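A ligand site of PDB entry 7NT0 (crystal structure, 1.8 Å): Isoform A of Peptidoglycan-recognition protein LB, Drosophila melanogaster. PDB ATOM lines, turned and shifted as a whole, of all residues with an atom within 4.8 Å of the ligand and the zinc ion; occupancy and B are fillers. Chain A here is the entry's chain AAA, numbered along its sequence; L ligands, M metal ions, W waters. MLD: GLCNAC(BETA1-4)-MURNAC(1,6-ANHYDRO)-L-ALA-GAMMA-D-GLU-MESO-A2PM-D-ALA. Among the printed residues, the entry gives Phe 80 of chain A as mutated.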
ATOM      1  N   ALA A   6      -3.284 -18.819   9.534  1.00  0.00           N
ATOM      2  CA  ALA A   6      -2.331 -18.772   8.411  1.00  0.00           C
ATOM      3  C   ALA A   6      -2.325 -17.380   7.767  1.00  0.00           C
ATOM      4  O   ALA A   6      -1.344 -17.133   7.048  1.00  0.00           O
ATOM      5  CB  ALA A   6      -2.730 -19.807   7.397  1.00  0.00           C
ATOM      6  N   ASN A   7      -3.414 -16.588   7.937  1.00  0.00           N
ATOM      7  CA  ASN A   7      -3.699 -15.411   7.056  1.00  0.00           C
ATOM      8  C   ASN A   7      -3.917 -14.138   7.857  1.00  0.00           C
ATOM      9  O   ASN A   7      -4.216 -13.147   7.216  1.00  0.00           O
ATOM     10  CB  ASN A   7      -4.885 -15.714   6.128  1.00  0.00           C
ATOM     11  CG  ASN A   7      -4.713 -17.095   5.547  1.00  0.00           C
ATOM     12  OD1 ASN A   7      -3.644 -17.411   5.027  1.00  0.00           O
ATOM     13  ND2 ASN A   7      -5.700 -17.963   5.733  1.00  0.00           N
ATOM     14  N   GLU A  32       7.617 -15.242  -9.398  1.00  0.00           N
ATOM     15  CA  GLU A  32       8.085 -16.364 -10.230  1.00  0.00           C
ATOM     16  C   GLU A  32       6.877 -16.901 -10.975  1.00  0.00           C
ATOM     17  O   GLU A  32       5.827 -17.064 -10.330  1.00  0.00           O
ATOM     18  CB  GLU A  32       8.692 -17.463  -9.377  1.00  0.00           C
ATOM     19  CG  GLU A  32       9.829 -17.012  -8.474  1.00  0.00           C
ATOM     20  CD  GLU A  32      10.289 -18.141  -7.550  1.00  0.00           C
ATOM     21  OE1 GLU A  32       9.662 -18.305  -6.477  1.00  0.00           O
ATOM     22  OE2 GLU A  32      11.225 -18.898  -7.933  1.00  0.00           O
ATOM     23  N   HIS A  44      -9.539 -22.681  -0.627  1.00  0.00           N
ATOM     24  CA  HIS A  44      -9.196 -22.334   0.748  1.00  0.00           C
ATOM     25  C   HIS A  44     -10.338 -21.524   1.337  1.00  0.00           C
ATOM     26  O   HIS A  44     -11.064 -20.859   0.579  1.00  0.00           O
ATOM     27  CB  HIS A  44      -7.918 -21.488   0.755  1.00  0.00           C
ATOM     28  CG  HIS A  44      -6.718 -22.133   0.163  1.00  0.00           C
ATOM     29  ND1 HIS A  44      -5.783 -22.823   0.906  1.00  0.00           N
ATOM     30  CD2 HIS A  44      -6.283 -22.179  -1.122  1.00  0.00           C
ATOM     31  CE1 HIS A  44      -4.811 -23.252   0.106  1.00  0.00           C
ATOM     32  NE2 HIS A  44      -5.102 -22.875  -1.154  1.00  0.00           N
ATOM     33  N   HIS A  45     -10.360 -21.431   2.683  1.00  0.00           N
ATOM     34  CA  HIS A  45     -11.044 -20.340   3.397  1.00  0.00           C
ATOM     35  C   HIS A  45      -9.999 -19.540   4.157  1.00  0.00           C
ATOM     36  O   HIS A  45      -8.900 -20.045   4.342  1.00  0.00           O
ATOM     37  CB  HIS A  45     -12.188 -20.816   4.278  1.00  0.00           C
ATOM     38  CG  HIS A  45     -11.760 -21.464   5.559  1.00  0.00           C
ATOM     39  ND1 HIS A  45     -12.646 -21.605   6.621  1.00  0.00           N
ATOM     40  CD2 HIS A  45     -10.639 -22.114   5.926  1.00  0.00           C
ATOM     41  CE1 HIS A  45     -12.018 -22.253   7.611  1.00  0.00           C
ATOM     42  NE2 HIS A  45     -10.809 -22.564   7.219  1.00  0.00           N
ATOM     43  N   SER A  46     -10.291 -18.313   4.522  1.00  0.00           N
ATOM     44  CA  SER A  46      -9.284 -17.497   5.263  1.00  0.00           C
ATOM     45  C   SER A  46      -9.256 -17.910   6.724  1.00  0.00           C
ATOM     46  O   SER A  46      -8.170 -17.760   7.338  1.00  0.00           O
ATOM     47  CB  SER A  46      -9.484 -16.014   5.066  1.00  0.00           C
ATOM     48  OG  SER A  46     -10.719 -15.566   5.573  1.00  0.00           O
ATOM     49  N   HIS A  69       1.157 -12.305   5.368  1.00  0.00           N
ATOM     50  CA  HIS A  69       2.011 -13.179   4.542  1.00  0.00           C
ATOM     51  C   HIS A  69       3.385 -12.535   4.289  1.00  0.00           C
ATOM     52  O   HIS A  69       4.428 -13.250   4.369  1.00  0.00           O
ATOM     53  CB  HIS A  69       1.265 -13.511   3.262  1.00  0.00           C
ATOM     54  CG  HIS A  69       0.098 -14.405   3.505  1.00  0.00           C
ATOM     55  ND1 HIS A  69      -0.725 -14.800   2.454  1.00  0.00           N
ATOM     56  CD2 HIS A  69      -0.341 -15.040   4.624  1.00  0.00           C
ATOM     57  CE1 HIS A  69      -1.686 -15.577   2.951  1.00  0.00           C
ATOM     58  NE2 HIS A  69      -1.444 -15.812   4.263  1.00  0.00           N
ATOM     59  N   ARG A  73       5.173 -13.770   7.719  1.00  0.00           N
ATOM     60  CA  ARG A  73       5.639 -15.086   7.211  1.00  0.00           C
ATOM     61  C   ARG A  73       6.849 -14.896   6.319  1.00  0.00           C
ATOM     62  O   ARG A  73       7.482 -15.928   6.004  1.00  0.00           O
ATOM     63  CB  ARG A  73       4.482 -15.846   6.555  1.00  0.00           C
ATOM     64  CG  ARG A  73       3.263 -15.886   7.484  1.00  0.00           C
ATOM     65  CD  ARG A  73       2.214 -16.904   7.084  1.00  0.00           C
ATOM     66  NE  ARG A  73       2.663 -18.288   7.178  1.00  0.00           N
ATOM     67  CZ  ARG A  73       1.869 -19.329   6.966  1.00  0.00           C
ATOM     68  NH1 ARG A  73       0.594 -19.126   6.652  1.00  0.00           N
ATOM     69  NH2 ARG A  73       2.350 -20.567   7.017  1.00  0.00           N
ATOM     70  N   TRP A  75       6.838 -14.001   3.139  1.00  0.00           N
ATOM     71  CA  TRP A  75       6.600 -14.425   1.753  1.00  0.00           C
ATOM     72  C   TRP A  75       6.700 -13.234   0.792  1.00  0.00           C
ATOM     73  O   TRP A  75       6.756 -12.044   1.227  1.00  0.00           O
ATOM     74  CB  TRP A  75       5.238 -15.118   1.665  1.00  0.00           C
ATOM     75  CG  TRP A  75       5.121 -16.360   2.478  1.00  0.00           C
ATOM     76  CD1 TRP A  75       6.083 -17.094   3.127  1.00  0.00           C
ATOM     77  CD2 TRP A  75       3.880 -17.038   2.738  1.00  0.00           C
ATOM     78  NE1 TRP A  75       5.526 -18.177   3.761  1.00  0.00           N
ATOM     79  CE2 TRP A  75       4.162 -18.158   3.542  1.00  0.00           C
ATOM     80  CE3 TRP A  75       2.563 -16.768   2.363  1.00  0.00           C
ATOM     81  CZ2 TRP A  75       3.165 -19.022   3.962  1.00  0.00           C
ATOM     82  CZ3 TRP A  75       1.589 -17.648   2.739  1.00  0.00           C
ATOM     83  CH2 TRP A  75       1.891 -18.738   3.563  1.00  0.00           C
ATOM     84  N   ASN A  76       6.743 -13.541  -0.485  1.00  0.00           N
ATOM     85  CA  ASN A  76       6.864 -12.568  -1.589  1.00  0.00           C
ATOM     86  C   ASN A  76       5.607 -11.725  -1.653  1.00  0.00           C
ATOM     87  O   ASN A  76       5.687 -10.568  -2.068  1.00  0.00           O
ATOM     88  CB  ASN A  76       7.110 -13.299  -2.898  1.00  0.00           C
ATOM     89  CG  ASN A  76       8.531 -13.822  -2.961  1.00  0.00           C
ATOM     90  OD1 ASN A  76       8.844 -14.768  -3.679  1.00  0.00           O
ATOM     91  ND2 ASN A  76       9.401 -13.162  -2.237  1.00  0.00           N
ATOM     92  N   ASP A  77       4.471 -12.301  -1.282  1.00  0.00           N
ATOM     93  CA  ASP A  77       3.180 -11.660  -1.600  1.00  0.00           C
ATOM     94  C   ASP A  77       2.108 -12.426  -0.816  1.00  0.00           C
ATOM     95  O   ASP A  77       2.437 -13.513  -0.227  1.00  0.00           O
ATOM     96  CB  ASP A  77       2.924 -11.713  -3.090  1.00  0.00           C
ATOM     97  CG  ASP A  77       1.798 -10.820  -3.590  1.00  0.00           C
ATOM     98  OD1 ASP A  77       1.329  -9.975  -2.809  1.00  0.00           O
ATOM     99  OD2 ASP A  77       1.393 -10.998  -4.770  1.00  0.00           O
ATOM    100  N   GLY A  79      -0.365 -15.192  -0.351  1.00  0.00           N
ATOM    101  CA  GLY A  79      -0.046 -16.555  -0.817  1.00  0.00           C
ATOM    102  C   GLY A  79      -0.984 -17.071  -1.913  1.00  0.00           C
ATOM    103  O   GLY A  79      -0.608 -18.008  -2.676  1.00  0.00           O
ATOM    104  N   PHE A  80      -2.209 -16.533  -1.951  1.00  0.00           N
ATOM    105  CA  PHE A  80      -3.298 -17.040  -2.821  1.00  0.00           C
ATOM    106  C   PHE A  80      -3.226 -16.385  -4.200  1.00  0.00           C
ATOM    107  O   PHE A  80      -2.773 -15.218  -4.369  1.00  0.00           O
ATOM    108  CB  PHE A  80      -4.640 -16.731  -2.190  1.00  0.00           C
ATOM    109  CG  PHE A  80      -4.807 -17.240  -0.791  1.00  0.00           C
ATOM    110  CD1 PHE A  80      -4.923 -18.588  -0.566  1.00  0.00           C
ATOM    111  CD2 PHE A  80      -4.888 -16.384   0.285  1.00  0.00           C
ATOM    112  CE1 PHE A  80      -5.123 -19.103   0.713  1.00  0.00           C
ATOM    113  CE2 PHE A  80      -5.077 -16.882   1.572  1.00  0.00           C
ATOM    114  CZ  PHE A  80      -5.172 -18.252   1.788  1.00  0.00           C
ATOM    115  N   ARG A  94      -1.870 -13.278  -6.344  1.00  0.00           N
ATOM    116  CA  ARG A  94      -0.720 -13.496  -7.256  1.00  0.00           C
ATOM    117  C   ARG A  94      -1.171 -13.634  -8.703  1.00  0.00           C
ATOM    118  O   ARG A  94      -0.363 -13.330  -9.585  1.00  0.00           O
ATOM    119  CB  ARG A  94       0.062 -14.733  -6.864  1.00  0.00           C
ATOM    120  CG  ARG A  94       0.593 -14.597  -5.449  1.00  0.00           C
ATOM    121  CD  ARG A  94       1.708 -15.547  -5.196  1.00  0.00           C
ATOM    122  NE  ARG A  94       2.173 -15.378  -3.841  1.00  0.00           N
ATOM    123  CZ  ARG A  94       3.321 -15.866  -3.354  1.00  0.00           C
ATOM    124  NH1 ARG A  94       4.122 -16.603  -4.106  1.00  0.00           N
ATOM    125  NH2 ARG A  94       3.673 -15.627  -2.108  1.00  0.00           N
ATOM    126  N   ILE A  99       3.650 -18.589  -9.327  1.00  0.00           N
ATOM    127  CA  ILE A  99       3.888 -19.591  -8.280  1.00  0.00           C
ATOM    128  C   ILE A  99       3.347 -19.024  -6.973  1.00  0.00           C
ATOM    129  O   ILE A  99       3.677 -17.884  -6.614  1.00  0.00           O
ATOM    130  CB  ILE A  99       5.390 -19.943  -8.175  1.00  0.00           C
ATOM    131  CG1 ILE A  99       5.899 -20.558  -9.494  1.00  0.00           C
ATOM    132  CG2 ILE A  99       5.596 -20.838  -6.971  1.00  0.00           C
ATOM    133  CD1 ILE A  99       7.346 -21.086  -9.437  1.00  0.00           C
ATOM    134  N   GLY A 100       2.477 -19.780  -6.332  1.00  0.00           N
ATOM    135  CA  GLY A 100       1.808 -19.352  -5.106  1.00  0.00           C
ATOM    136  C   GLY A 100       2.563 -19.747  -3.844  1.00  0.00           C
ATOM    137  O   GLY A 100       3.694 -20.295  -3.902  1.00  0.00           O
ATOM    138  N   ALA A 101       1.933 -19.455  -2.727  1.00  0.00           N
ATOM    139  CA  ALA A 101       2.370 -19.814  -1.367  1.00  0.00           C
ATOM    140  C   ALA A 101       1.115 -20.179  -0.587  1.00  0.00           C
ATOM    141  O   ALA A 101       0.794 -19.524   0.385  1.00  0.00           O
ATOM    142  CB  ALA A 101       3.137 -18.679  -0.742  1.00  0.00           C
ATOM    143  N   HIS A 102       0.381 -21.180  -1.071  1.00  0.00           N
ATOM    144  CA  HIS A 102      -0.889 -21.614  -0.439  1.00  0.00           C
ATOM    145  C   HIS A 102      -0.970 -23.128  -0.252  1.00  0.00           C
ATOM    146  O   HIS A 102      -1.716 -23.521   0.640  1.00  0.00           O
ATOM    147  CB  HIS A 102      -2.067 -21.022  -1.243  1.00  0.00           C
ATOM    148  CG  HIS A 102      -2.128 -21.558  -2.623  1.00  0.00           C
ATOM    149  ND1 HIS A 102      -2.870 -22.660  -2.916  1.00  0.00           N
ATOM    150  CD2 HIS A 102      -1.579 -21.137  -3.798  1.00  0.00           C
ATOM    151  CE1 HIS A 102      -2.713 -22.956  -4.184  1.00  0.00           C
ATOM    152  NE2 HIS A 102      -1.904 -22.042  -4.751  1.00  0.00           N
ATOM    153  N   ALA A 103      -0.239 -23.938  -1.002  1.00  0.00           N
ATOM    154  CA  ALA A 103      -0.323 -25.410  -0.935  1.00  0.00           C
ATOM    155  C   ALA A 103       0.979 -26.034  -1.432  1.00  0.00           C
ATOM    156  O   ALA A 103       1.195 -26.131  -2.630  1.00  0.00           O
ATOM    157  CB  ALA A 103      -1.495 -25.905  -1.738  1.00  0.00           C
ATOM    158  N   PRO A 104       1.878 -26.420  -0.509  1.00  0.00           N
ATOM    159  CA  PRO A 104       3.178 -26.999  -0.885  1.00  0.00           C
ATOM    160  C   PRO A 104       3.023 -28.196  -1.832  1.00  0.00           C
ATOM    161  O   PRO A 104       2.051 -28.965  -1.668  1.00  0.00           O
ATOM    162  CB  PRO A 104       3.797 -27.407   0.468  1.00  0.00           C
ATOM    163  CG  PRO A 104       3.168 -26.455   1.454  1.00  0.00           C
ATOM    164  CD  PRO A 104       1.739 -26.258   0.949  1.00  0.00           C
ATOM    165  N   LYS A 105       3.895 -28.246  -2.839  1.00  0.00           N
ATOM    166  CA  LYS A 105       3.950 -29.253  -3.929  1.00  0.00           C
ATOM    167  C   LYS A 105       2.916 -28.901  -5.002  1.00  0.00           C
ATOM    168  O   LYS A 105       2.936 -29.500  -6.061  1.00  0.00           O
ATOM    169  CB  LYS A 105       3.784 -30.670  -3.328  1.00  0.00           C
ATOM    170  N   ASN A 107       2.050 -25.331  -5.564  1.00  0.00           N
ATOM    171  CA  ASN A 107       2.137 -23.881  -5.758  1.00  0.00           C
ATOM    172  C   ASN A 107       2.528 -23.540  -7.188  1.00  0.00           C
ATOM    173  O   ASN A 107       2.174 -22.426  -7.656  1.00  0.00           O
ATOM    174  CB  ASN A 107       3.111 -23.281  -4.770  1.00  0.00           C
ATOM    175  CG  ASN A 107       2.526 -23.180  -3.386  1.00  0.00           C
ATOM    176  OD1 ASN A 107       1.348 -22.843  -3.193  1.00  0.00           O
ATOM    177  ND2 ASN A 107       3.350 -23.466  -2.403  1.00  0.00           N
ATOM    178  N   HIS A 154      -7.858 -27.590   0.120  1.00  0.00           N
ATOM    179  CA  HIS A 154      -6.515 -27.595   0.743  1.00  0.00           C
ATOM    180  C   HIS A 154      -6.301 -28.897   1.570  1.00  0.00           C
ATOM    181  O   HIS A 154      -5.205 -29.482   1.479  1.00  0.00           O
ATOM    182  CB  HIS A 154      -6.331 -26.327   1.570  1.00  0.00           C
ATOM    183  CG  HIS A 154      -4.930 -26.079   2.001  1.00  0.00           C
ATOM    184  ND1 HIS A 154      -4.615 -25.030   2.793  1.00  0.00           N
ATOM    185  CD2 HIS A 154      -3.774 -26.764   1.772  1.00  0.00           C
ATOM    186  CE1 HIS A 154      -3.314 -25.041   3.071  1.00  0.00           C
ATOM    187  NE2 HIS A 154      -2.757 -26.091   2.398  1.00  0.00           N
ATOM    188  N   ARG A 158      -2.742 -31.338   2.357  1.00  0.00           N
ATOM    189  CA  ARG A 158      -1.980 -30.842   3.531  1.00  0.00           C
ATOM    190  C   ARG A 158      -2.859 -31.169   4.734  1.00  0.00           C
ATOM    191  O   ARG A 158      -4.098 -31.203   4.601  1.00  0.00           O
ATOM    192  CB  ARG A 158      -1.675 -29.336   3.405  1.00  0.00           C
ATOM    193  N   CYS A 162      -8.731 -26.433   6.497  1.00  0.00           N
ATOM    194  CA  CYS A 162      -8.997 -25.558   5.316  1.00  0.00           C
ATOM    195  C   CYS A 162      -9.530 -26.442   4.181  1.00  0.00           C
ATOM    196  O   CYS A 162      -8.895 -27.451   3.859  1.00  0.00           O
ATOM    197  CB  CYS A 162      -7.712 -24.843   4.955  1.00  0.00           C
ATOM    198  SG  CYS A 162      -7.984 -23.615   3.635  1.00  0.00           S
HETATM  199  CAI MLD L   1      -5.615 -20.646   4.845  1.00  0.00           C
HETATM  200  CAL MLD L   1      -4.440 -21.153   4.107  1.00  0.00           C
HETATM  201  OAM MLD L   1      -4.428 -22.317   3.754  1.00  0.00           O
HETATM  202  N   MLD L   1      -3.439 -20.284   3.970  1.00  0.00           N
HETATM  203  CA  MLD L   1      -2.280 -20.589   3.170  1.00  0.00           C
HETATM  204  CB  MLD L   1      -1.681 -19.314   2.592  1.00  0.00           C
HETATM  205  C   MLD L   1      -1.198 -21.364   3.928  1.00  0.00           C
HETATM  206  O   MLD L   1      -0.787 -20.965   5.002  1.00  0.00           O
HETATM  207  NAN MLD L   1      -0.750 -22.460   3.330  1.00  0.00           N
HETATM  208  CAO MLD L   1       0.555 -23.002   3.598  1.00  0.00           C
HETATM  209  CAP MLD L   1       0.495 -24.499   4.004  1.00  0.00           C
HETATM  210  OBA MLD L   1       1.148 -24.828   4.965  1.00  0.00           O
HETATM  211  OAQ MLD L   1      -0.271 -25.282   3.395  1.00  0.00           O
HETATM  212  CBB MLD L   1       1.413 -22.654   2.403  1.00  0.00           C
HETATM  213  CBC MLD L   1       2.866 -22.634   2.725  1.00  0.00           C
HETATM  214  CBD MLD L   1       3.606 -22.464   1.435  1.00  0.00           C
HETATM  215  OBE MLD L   1       3.202 -22.926   0.366  1.00  0.00           O
HETATM  216  NBF MLD L   1       4.740 -21.776   1.560  1.00  0.00           N
HETATM  217  CBG MLD L   1       5.645 -21.656   0.447  1.00  0.00           C
HETATM  218  CBH MLD L   1       6.280 -23.017   0.095  1.00  0.00           C
HETATM  219  OBI MLD L   1       6.417 -23.849   0.984  1.00  0.00           O
HETATM  220  NBJ MLD L   1       6.579 -23.295  -1.185  1.00  0.00           N
HETATM  221  CBK MLD L   1       7.197 -24.563  -1.621  1.00  0.00           C
HETATM  222  CBL MLD L   1       8.441 -24.286  -2.465  1.00  0.00           C
HETATM  223  CBM MLD L   1       6.296 -25.484  -2.494  1.00  0.00           C
HETATM  224  OBO MLD L   1       5.601 -24.967  -3.375  1.00  0.00           O
HETATM  225  OBN MLD L   1       6.389 -26.706  -2.313  1.00  0.00           O
HETATM  226  CBP MLD L   1       6.604 -20.539   0.859  1.00  0.00           C
HETATM  227  CBQ MLD L   1       6.986 -19.710  -0.321  1.00  0.00           C
HETATM  228  CBR MLD L   1       7.787 -18.461  -0.016  1.00  0.00           C
HETATM  229  CBS MLD L   1       8.144 -17.684  -1.279  1.00  0.00           C
HETATM  230  CBT MLD L   1       6.870 -17.103  -1.931  1.00  0.00           C
HETATM  231  OBV MLD L   1       6.223 -16.248  -1.298  1.00  0.00           O
HETATM  232  OBU MLD L   1       6.624 -17.482  -3.076  1.00  0.00           O
HETATM  233  NBW MLD L   1       8.826 -18.593  -2.233  1.00  0.00           N
HETATM  234 ZN    ZN M   1      -5.876 -23.333   2.925  1.00  0.00          ZN
HETATM  235  O   HOH W   1       6.097 -21.396  -3.244  1.00  0.00           O
HETATM  236  O   HOH W   2      -4.084 -23.674   6.670  1.00  0.00           O
HETATM  237  O   HOH W   3       4.888 -26.204  -5.574  1.00  0.00           O
HETATM  238  O   HOH W   4       0.786 -22.844   7.262  1.00  0.00           O
HETATM  239  O   HOH W   5       5.855 -21.314   4.198  1.00  0.00           O
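The zinc ion is bound by OAM of the ligand (2.0 Å), ND1 of His 44 (2.1 Å), ND1 of His 154 (2.1 Å) and SG of Cys 162 (2.2 Å).
The guanidinium group (NH2) of Arg 94 is in salt-bridge range of an oxygen (OBV) of the ligand (2.7 Å).
The side-chain amide nitrogen (ND2) of Asn 107 lies within hydrogen-bond range of an oxygen (OBE) of the ligand, 2.8 Å away.
OD1 of Asn 7 sits at hydrogen-bond distance from N of the ligand, at 3.1 Å.
NH1 of Arg 73 lies within hydrogen-bond range of O of the ligand.
The backbone NH of Asn 76 sits at hydrogen-bond distance from an oxygen (OBV) of the ligand (2.9 Å).
The backbone NH (N) of Lys 105 lies within hydrogen-bond range of an oxygen (OBN) of the ligand, 3.0 Å away.
The backbone carbonyl oxygen of His 102 sits at hydrogen-bond distance from a nitrogen (NAN) of the ligand, at 3.0 Å.
A ring nitrogen (NE2) of His 44 sits at hydrogen-bond distance from a ring nitrogen (ND1) of His 102 (2.9 Å).
The backbone carbonyl oxygen of His 102 lies close to a ring nitrogen (NE2) of His 154 (3.3 Å).
The guanidinium group (NH1) of Arg 94 is in hydrogen-bond range of the backbone carbonyl oxygen (O) of Ile 99 (2.9 Å).
The side-chain amide oxygen (OD1) of Asn 107 lies within hydrogen-bond range of the backbone NH (N) of His 102 (2.9 Å).
The side-chain amide oxygen of Asn 107 lies within hydrogen-bond range of the backbone NH of Ala 103.
ND2 of Asn 7 sits at hydrogen-bond distance from O of Ser 46 (3.0 Å).
The backbone carbonyl oxygen of His 69 lies within hydrogen-bond range of the backbone NH of Trp 75, 2.8 Å away.
N of Ala 101 is in hydrogen-bond range of O of Gly 79 (2.9 Å).
Water W3 lies within hydrogen-bond range of OBO of the ligand (2.6 Å) and N of Asn 107 (3.0 Å).
Water W1 bridges O of Gly 100 and NBJ of the ligand.
Water W5 bridges NBF of the ligand and NE1 of Trp 75.
Water W4 bridges NH2 of Arg 73 and OBA of the ligand.
Ala 6 touches the ligand (CB to O, 3.3 Å).
His 45 touches the ligand (O to CAI, 3.4 Å).
His 69 touches the ligand (CE1 to CB, 3.8 Å).
Trp 75 touches the ligand (CB to OBV, 3.3 Å).
Phe 80 touches the ligand.
Ala 101 touches the ligand.
Ala 103 touches the ligand (N to OBE, 3.8 Å).
Pro 104 touches the ligand.
Hydrophobic or aromatic side chains that line the ligand: Ala 6, His 44, His 69, Trp 75, Phe 80, Ala 101, Pro 104 and His 154.
Of the 25 residues printed, 18 come within 4 Å of the ligand.
The nearest printed residue that does not touch the ligand is Gly 100 (4.1 Å).
Within 4 Å of the zinc ion: His 44, His 154 and Cys 162.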
